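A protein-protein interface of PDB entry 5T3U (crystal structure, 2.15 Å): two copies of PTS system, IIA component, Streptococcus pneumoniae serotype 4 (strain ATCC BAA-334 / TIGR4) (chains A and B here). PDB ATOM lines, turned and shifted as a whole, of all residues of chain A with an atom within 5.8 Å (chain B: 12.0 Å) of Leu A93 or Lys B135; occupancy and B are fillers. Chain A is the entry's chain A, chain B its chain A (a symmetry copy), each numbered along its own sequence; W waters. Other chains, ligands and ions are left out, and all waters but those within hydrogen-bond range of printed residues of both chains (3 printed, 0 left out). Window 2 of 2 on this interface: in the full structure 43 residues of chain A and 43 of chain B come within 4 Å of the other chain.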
ATOM      1  N   LEU A  65      -5.030 -33.069  -0.807  1.00  0.00           N
ATOM      2  CA  LEU A  65      -4.263 -33.653   0.312  1.00  0.00           C
ATOM      3  C   LEU A  65      -4.537 -35.144   0.587  1.00  0.00           C
ATOM      4  O   LEU A  65      -3.707 -35.825   1.250  1.00  0.00           O
ATOM      5  CB  LEU A  65      -4.365 -32.813   1.603  1.00  0.00           C
ATOM      6  CG  LEU A  65      -3.667 -31.442   1.643  1.00  0.00           C
ATOM      7  CD1 LEU A  65      -4.272 -30.556   2.757  1.00  0.00           C
ATOM      8  CD2 LEU A  65      -2.142 -31.556   1.786  1.00  0.00           C
ATOM      9  N   LEU A  87      -5.217 -18.086   2.495  1.00  0.00           N
ATOM     10  CA  LEU A  87      -4.438 -17.726   3.657  1.00  0.00           C
ATOM     11  C   LEU A  87      -5.247 -17.932   4.956  1.00  0.00           C
ATOM     12  O   LEU A  87      -4.720 -18.466   5.932  1.00  0.00           O
ATOM     13  CB  LEU A  87      -3.939 -16.278   3.559  1.00  0.00           C
ATOM     14  CG  LEU A  87      -2.970 -15.835   4.667  1.00  0.00           C
ATOM     15  CD1 LEU A  87      -1.657 -16.586   4.637  1.00  0.00           C
ATOM     16  CD2 LEU A  87      -2.699 -14.327   4.585  1.00  0.00           C
ATOM     17  N   PHE A  90      -5.999 -21.943   5.433  1.00  0.00           N
ATOM     18  CA  PHE A  90      -4.842 -22.827   5.630  1.00  0.00           C
ATOM     19  C   PHE A  90      -3.633 -22.167   6.274  1.00  0.00           C
ATOM     20  O   PHE A  90      -2.512 -22.658   6.138  1.00  0.00           O
ATOM     21  CB  PHE A  90      -4.483 -23.526   4.302  1.00  0.00           C
ATOM     22  CG  PHE A  90      -5.622 -24.380   3.759  1.00  0.00           C
ATOM     23  CD1 PHE A  90      -5.940 -25.603   4.362  1.00  0.00           C
ATOM     24  CD2 PHE A  90      -6.400 -23.938   2.704  1.00  0.00           C
ATOM     25  CE1 PHE A  90      -6.997 -26.389   3.893  1.00  0.00           C
ATOM     26  CE2 PHE A  90      -7.468 -24.707   2.224  1.00  0.00           C
ATOM     27  CZ  PHE A  90      -7.761 -25.939   2.821  1.00  0.00           C
ATOM     28  N   LEU A  91      -3.882 -21.076   7.008  1.00  0.00           N
ATOM     29  CA  LEU A  91      -2.841 -20.242   7.603  1.00  0.00           C
ATOM     30  C   LEU A  91      -1.689 -21.015   8.229  1.00  0.00           C
ATOM     31  O   LEU A  91      -0.531 -20.746   7.920  1.00  0.00           O
ATOM     32  CB  LEU A  91      -3.434 -19.286   8.652  1.00  0.00           C
ATOM     33  CG  LEU A  91      -2.442 -18.325   9.324  1.00  0.00           C
ATOM     34  CD1 LEU A  91      -1.783 -17.376   8.292  1.00  0.00           C
ATOM     35  CD2 LEU A  91      -3.115 -17.551  10.451  1.00  0.00           C
ATOM     36  N   ASN A  92      -2.013 -21.957   9.125  1.00  0.00           N
ATOM     37  CA  ASN A  92      -0.996 -22.670   9.877  1.00  0.00           C
ATOM     38  C   ASN A  92      -0.827 -24.123   9.438  1.00  0.00           C
ATOM     39  O   ASN A  92      -0.106 -24.880  10.103  1.00  0.00           O
ATOM     40  CB  ASN A  92      -1.263 -22.592  11.396  1.00  0.00           C
ATOM     41  CG  ASN A  92      -1.147 -21.168  11.960  1.00  0.00           C
ATOM     42  OD1 ASN A  92      -1.993 -20.729  12.751  1.00  0.00           O
ATOM     43  ND2 ASN A  92      -0.123 -20.455  11.560  1.00  0.00           N
ATOM     44  N   LEU A  93      -1.484 -24.530   8.343  1.00  0.00           N
ATOM     45  CA  LEU A  93      -1.243 -25.868   7.808  1.00  0.00           C
ATOM     46  C   LEU A  93       0.029 -25.910   6.964  1.00  0.00           C
ATOM     47  O   LEU A  93       0.047 -25.452   5.807  1.00  0.00           O
ATOM     48  CB  LEU A  93      -2.448 -26.390   7.036  1.00  0.00           C
ATOM     49  CG  LEU A  93      -2.421 -27.868   6.605  1.00  0.00           C
ATOM     50  CD1 LEU A  93      -2.126 -28.842   7.768  1.00  0.00           C
ATOM     51  CD2 LEU A  93      -3.728 -28.234   5.955  1.00  0.00           C
ATOM     52  N   ASP A  94       1.109 -26.422   7.553  1.00  0.00           N
ATOM     53  CA  ASP A  94       2.401 -26.423   6.891  1.00  0.00           C
ATOM     54  C   ASP A  94       2.448 -27.197   5.561  1.00  0.00           C
ATOM     55  O   ASP A  94       3.286 -26.896   4.708  1.00  0.00           O
ATOM     56  CB  ASP A  94       3.479 -26.963   7.826  1.00  0.00           C
ATOM     57  CG  ASP A  94       3.802 -26.013   8.979  1.00  0.00           C
ATOM     58  OD1 ASP A  94       3.432 -24.808   8.941  1.00  0.00           O
ATOM     59  OD2 ASP A  94       4.429 -26.495   9.942  1.00  0.00           O
ATOM     60  N   SER A  95       1.566 -28.179   5.387  1.00  0.00           N
ATOM     61  CA  SER A  95       1.537 -28.958   4.144  1.00  0.00           C
ATOM     62  C   SER A  95       0.956 -28.149   2.959  1.00  0.00           C
ATOM     63  O   SER A  95       0.969 -28.618   1.819  1.00  0.00           O
ATOM     64  CB  SER A  95       0.720 -30.215   4.322  1.00  0.00           C
ATOM     65  OG  SER A  95      -0.598 -29.836   4.655  1.00  0.00           O
ATOM     66  N   VAL A  96       0.456 -26.947   3.227  1.00  0.00           N
ATOM     67  CA  VAL A  96      -0.129 -26.126   2.155  1.00  0.00           C
ATOM     68  C   VAL A  96       0.679 -24.860   1.986  1.00  0.00           C
ATOM     69  O   VAL A  96       0.747 -24.039   2.901  1.00  0.00           O
ATOM     70  CB  VAL A  96      -1.595 -25.755   2.432  1.00  0.00           C
ATOM     71  CG1 VAL A  96      -2.127 -24.766   1.368  1.00  0.00           C
ATOM     72  CG2 VAL A  96      -2.465 -27.009   2.486  1.00  0.00           C
ATOM     73  N   ASP A  97       1.296 -24.717   0.813  1.00  0.00           N
ATOM     74  CA  ASP A  97       1.971 -23.477   0.474  1.00  0.00           C
ATOM     75  C   ASP A  97       1.119 -22.600  -0.424  1.00  0.00           C
ATOM     76  O   ASP A  97       0.288 -23.103  -1.172  1.00  0.00           O
ATOM     77  CB  ASP A  97       3.323 -23.754  -0.183  1.00  0.00           C
ATOM     78  CG  ASP A  97       4.350 -24.213   0.821  1.00  0.00           C
ATOM     79  OD1 ASP A  97       4.584 -23.458   1.792  1.00  0.00           O
ATOM     80  OD2 ASP A  97       4.885 -25.337   0.655  1.00  0.00           O
ATOM     81  N   ILE A  98       1.342 -21.287  -0.333  1.00  0.00           N
ATOM     82  CA  ILE A  98       0.593 -20.311  -1.134  1.00  0.00           C
ATOM     83  C   ILE A  98       1.564 -19.370  -1.844  1.00  0.00           C
ATOM     84  O   ILE A  98       2.308 -18.643  -1.187  1.00  0.00           O
ATOM     85  CB  ILE A  98      -0.403 -19.475  -0.274  1.00  0.00           C
ATOM     86  CG1 ILE A  98      -1.316 -20.404   0.565  1.00  0.00           C
ATOM     87  CG2 ILE A  98      -1.222 -18.522  -1.206  1.00  0.00           C
ATOM     88  CD1 ILE A  98      -2.099 -19.691   1.649  1.00  0.00           C
ATOM     89  N   ASN B 129       8.090  -8.552  -8.169  1.00  0.00           N
ATOM     90  CA  ASN B 129       7.916  -8.576  -6.732  1.00  0.00           C
ATOM     91  C   ASN B 129       6.522  -8.990  -6.328  1.00  0.00           C
ATOM     92  O   ASN B 129       6.313  -9.303  -5.170  1.00  0.00           O
ATOM     93  CB  ASN B 129       8.209  -7.199  -6.128  1.00  0.00           C
ATOM     94  CG  ASN B 129       9.717  -6.905  -6.000  1.00  0.00           C
ATOM     95  OD1 ASN B 129      10.560  -7.811  -6.035  1.00  0.00           O
ATOM     96  ND2 ASN B 129      10.049  -5.624  -5.834  1.00  0.00           N
ATOM     97  N   SER B 130       5.563  -8.920  -7.265  1.00  0.00           N
ATOM     98  CA  SER B 130       4.191  -9.397  -7.041  1.00  0.00           C
ATOM     99  C   SER B 130       4.020 -10.927  -7.119  1.00  0.00           C
ATOM    100  O   SER B 130       2.962 -11.453  -6.762  1.00  0.00           O
ATOM    101  CB  SER B 130       3.253  -8.777  -8.039  1.00  0.00           C
ATOM    102  OG  SER B 130       3.123  -7.382  -7.810  1.00  0.00           O
ATOM    103  N   LEU B 131       5.031 -11.618  -7.618  1.00  0.00           N
ATOM    104  CA  LEU B 131       5.085 -13.069  -7.571  1.00  0.00           C
ATOM    105  C   LEU B 131       5.884 -13.473  -6.326  1.00  0.00           C
ATOM    106  O   LEU B 131       7.102 -13.268  -6.274  1.00  0.00           O
ATOM    107  CB  LEU B 131       5.749 -13.614  -8.834  1.00  0.00           C
ATOM    108  CG  LEU B 131       5.635 -15.127  -9.125  1.00  0.00           C
ATOM    109  CD1 LEU B 131       6.044 -15.431 -10.577  1.00  0.00           C
ATOM    110  CD2 LEU B 131       6.469 -15.964  -8.151  1.00  0.00           C
ATOM    111  N   PHE B 132       5.206 -14.023  -5.314  1.00  0.00           N
ATOM    112  CA  PHE B 132       5.905 -14.359  -4.094  1.00  0.00           C
ATOM    113  C   PHE B 132       5.205 -15.393  -3.219  1.00  0.00           C
ATOM    114  O   PHE B 132       3.999 -15.567  -3.291  1.00  0.00           O
ATOM    115  CB  PHE B 132       6.203 -13.084  -3.256  1.00  0.00           C
ATOM    116  CG  PHE B 132       4.962 -12.353  -2.770  1.00  0.00           C
ATOM    117  CD1 PHE B 132       4.352 -11.382  -3.568  1.00  0.00           C
ATOM    118  CD2 PHE B 132       4.433 -12.611  -1.501  1.00  0.00           C
ATOM    119  CE1 PHE B 132       3.219 -10.658  -3.095  1.00  0.00           C
ATOM    120  CE2 PHE B 132       3.317 -11.914  -1.030  1.00  0.00           C
ATOM    121  CZ  PHE B 132       2.701 -10.935  -1.828  1.00  0.00           C
ATOM    122  N   ASN B 133       5.985 -16.031  -2.351  1.00  0.00           N
ATOM    123  CA  ASN B 133       5.455 -17.001  -1.395  1.00  0.00           C
ATOM    124  C   ASN B 133       4.782 -16.198  -0.289  1.00  0.00           C
ATOM    125  O   ASN B 133       5.450 -15.437   0.429  1.00  0.00           O
ATOM    126  CB  ASN B 133       6.615 -17.851  -0.879  1.00  0.00           C
ATOM    127  CG  ASN B 133       6.219 -18.842   0.208  1.00  0.00           C
ATOM    128  OD1 ASN B 133       5.347 -18.581   1.042  1.00  0.00           O
ATOM    129  ND2 ASN B 133       6.891 -19.989   0.216  1.00  0.00           N
ATOM    130  N   VAL B 134       3.467 -16.323  -0.160  1.00  0.00           N
ATOM    131  CA  VAL B 134       2.783 -15.413   0.746  1.00  0.00           C
ATOM    132  C   VAL B 134       2.991 -15.674   2.253  1.00  0.00           C
ATOM    133  O   VAL B 134       3.029 -14.717   3.018  1.00  0.00           O
ATOM    134  CB  VAL B 134       1.293 -15.110   0.353  1.00  0.00           C
ATOM    135  CG1 VAL B 134       1.003 -15.396  -1.140  1.00  0.00           C
ATOM    136  CG2 VAL B 134       0.283 -15.750   1.280  1.00  0.00           C
ATOM    137  N   LYS B 135       3.172 -16.935   2.663  1.00  0.00           N
ATOM    138  CA  LYS B 135       3.417 -17.251   4.081  1.00  0.00           C
ATOM    139  C   LYS B 135       4.812 -16.791   4.485  1.00  0.00           C
ATOM    140  O   LYS B 135       4.992 -16.202   5.547  1.00  0.00           O
ATOM    141  CB  LYS B 135       3.247 -18.750   4.354  1.00  0.00           C
ATOM    142  CG  LYS B 135       1.821 -19.257   4.233  1.00  0.00           C
ATOM    143  CD  LYS B 135       1.776 -20.765   4.544  1.00  0.00           C
ATOM    144  CE  LYS B 135       0.351 -21.211   4.818  1.00  0.00           C
ATOM    145  NZ  LYS B 135       0.243 -22.635   5.200  1.00  0.00           N
ATOM    146  N   GLN B 136       5.792 -17.029   3.610  1.00  0.00           N
ATOM    147  CA  GLN B 136       7.154 -16.556   3.835  1.00  0.00           C
ATOM    148  C   GLN B 136       7.188 -15.044   3.999  1.00  0.00           C
ATOM    149  O   GLN B 136       7.832 -14.535   4.901  1.00  0.00           O
ATOM    150  CB  GLN B 136       8.077 -16.968   2.698  1.00  0.00           C
ATOM    151  CG  GLN B 136       9.564 -16.696   2.949  1.00  0.00           C
ATOM    152  CD  GLN B 136      10.433 -16.831   1.672  1.00  0.00           C
ATOM    153  OE1 GLN B 136      10.101 -17.583   0.752  1.00  0.00           O
ATOM    154  NE2 GLN B 136      11.548 -16.098   1.628  1.00  0.00           N
ATOM    155  N   GLN B 137       6.493 -14.330   3.130  1.00  0.00           N
ATOM    156  CA  GLN B 137       6.581 -12.883   3.138  1.00  0.00           C
ATOM    157  C   GLN B 137       5.765 -12.256   4.256  1.00  0.00           C
ATOM    158  O   GLN B 137       6.147 -11.216   4.774  1.00  0.00           O
ATOM    159  CB  GLN B 137       6.159 -12.286   1.799  1.00  0.00           C
ATOM    160  CG  GLN B 137       6.468 -10.781   1.686  1.00  0.00           C
ATOM    161  CD  GLN B 137       6.551 -10.309   0.236  1.00  0.00           C
ATOM    162  OE1 GLN B 137       7.404 -10.775  -0.546  1.00  0.00           O
ATOM    163  NE2 GLN B 137       5.666  -9.372  -0.127  1.00  0.00           N
ATOM    164  N   LEU B 138       4.638 -12.873   4.605  1.00  0.00           N
ATOM    165  CA  LEU B 138       3.774 -12.332   5.651  1.00  0.00           C
ATOM    166  C   LEU B 138       4.221 -12.816   7.029  1.00  0.00           C
ATOM    167  O   LEU B 138       3.737 -12.322   8.057  1.00  0.00           O
ATOM    168  CB  LEU B 138       2.289 -12.631   5.365  1.00  0.00           C
ATOM    169  CG  LEU B 138       1.589 -11.695   4.349  1.00  0.00           C
ATOM    170  CD1 LEU B 138       2.253 -11.620   2.935  1.00  0.00           C
ATOM    171  CD2 LEU B 138       0.115 -12.044   4.194  1.00  0.00           C
ATOM    172  N   ASN B 139       5.174 -13.751   7.022  1.00  0.00           N
ATOM    173  CA  ASN B 139       5.836 -14.326   8.217  1.00  0.00           C
ATOM    174  C   ASN B 139       4.944 -15.253   9.067  1.00  0.00           C
ATOM    175  O   ASN B 139       4.367 -16.234   8.554  1.00  0.00           O
ATOM    176  CB  ASN B 139       6.515 -13.235   9.060  1.00  0.00           C
ATOM    177  CG  ASN B 139       7.834 -12.762   8.456  1.00  0.00           C
ATOM    178  OD1 ASN B 139       8.905 -13.292   8.769  1.00  0.00           O
ATOM    179  ND2 ASN B 139       7.763 -11.745   7.605  1.00  0.00           N
HETATM  180  O   HOH W   1       6.764 -22.002   2.231  1.00  0.00           O
HETATM  181  O   HOH W   2       3.443 -20.674   1.501  1.00  0.00           O
HETATM  182  O   HOH W   3       1.820 -22.952   7.567  1.00  0.00           O
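NZ of Lys B135 is in hydrogen-bond range of O of Phe A90 (2.9 Å).
NZ of Lys B135 sits close to O of Leu A91 (3.4 Å).
NZ of Lys B135 sits at hydrogen-bond distance from O of Leu A93 (2.9 Å).
O of Val A96 lies within hydrogen-bond range of NZ of Lys B135 (2.7 Å).
The backbone NH (N) of Val B134 sits at hydrogen-bond distance from the backbone carbonyl oxygen (O) of Ile A98.
N of Lys B135 sits at hydrogen-bond distance from OD1 of Asn B133 (3.2 Å).
The backbone NH (N) of Gln B136 lies within hydrogen-bond range of the side-chain amide oxygen (OD1) of Asn B133, at 3.0 Å.
Among the printed residues, merely in contact across the chains: Leu A87 with Val B134 (3.97 Å), Leu A87 with Leu B138 (3.6 Å) and Ile A98 with Asn B133 (3.6 Å).
Leu A87 touches just these residues of chain B: Val B134 and Leu B138.
Of chain B, only Lys B135 comes within 4 Å of Phe A90.
Of the printed residues of chain B, Leu A91 touches Lys B135.
No residue of chain B comes within 4 Å of Asp A94.
No residue of chain B comes within 4 Å of Ser A95.
No residue of chain B comes within 4 Å of Asp A97.
Of chain B, only Asn B133 and Val B134 come within 4 Å of Ile A98.
Of the printed residues of chain A, Asn B133 touches Ile A98 (3.6 Å).
Of the printed residues of chain A, Val B134 touches Leu A87 (3.97 Å) and Ile A98 (2.8 Å).
Printed residues of chain A within 4 Å of Leu B138: Leu A87 (3.6 Å).
The nearest printed residue of chain A that does not touch Val B134 is Asp A97 (6.7 Å).
Of the 11 printed residues of chain B, 4 touch a printed residue of chain A.
Printed residues of chain B that touch a printed residue of chain A: Asn B133, Val B134, Lys B135 and Leu B138.
Hydrophobic or aromatic side chains of chain B that line the printed part of chain A: Val B134 and Leu B138.
Hydrophobic or aromatic side chains of chain A that line the printed part of chain B: Leu A87 and Ile A98.
No position is printed for both chains.
Of the 8 pairs that touch across the chains among the printed residues, none has its exchanged pair printed and touching as well.
Water W1 bridges the side-chain carboxylate of Asp A97 and the side-chain amide nitrogen of Asn B133.
Water W3 lies within hydrogen-bond range of OD1 of Asp A94 (2.8 Å), NZ of Lys B135 (2.9 Å) and O of Leu A91 (3.2 Å).
Water W2 lies within hydrogen-bond range of the backbone NH of Ile A98 (2.9 Å), the side-chain amide oxygen of Asn B133 (2.9 Å) and the side-chain carboxylate of Asp A97 (3.0 Å).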
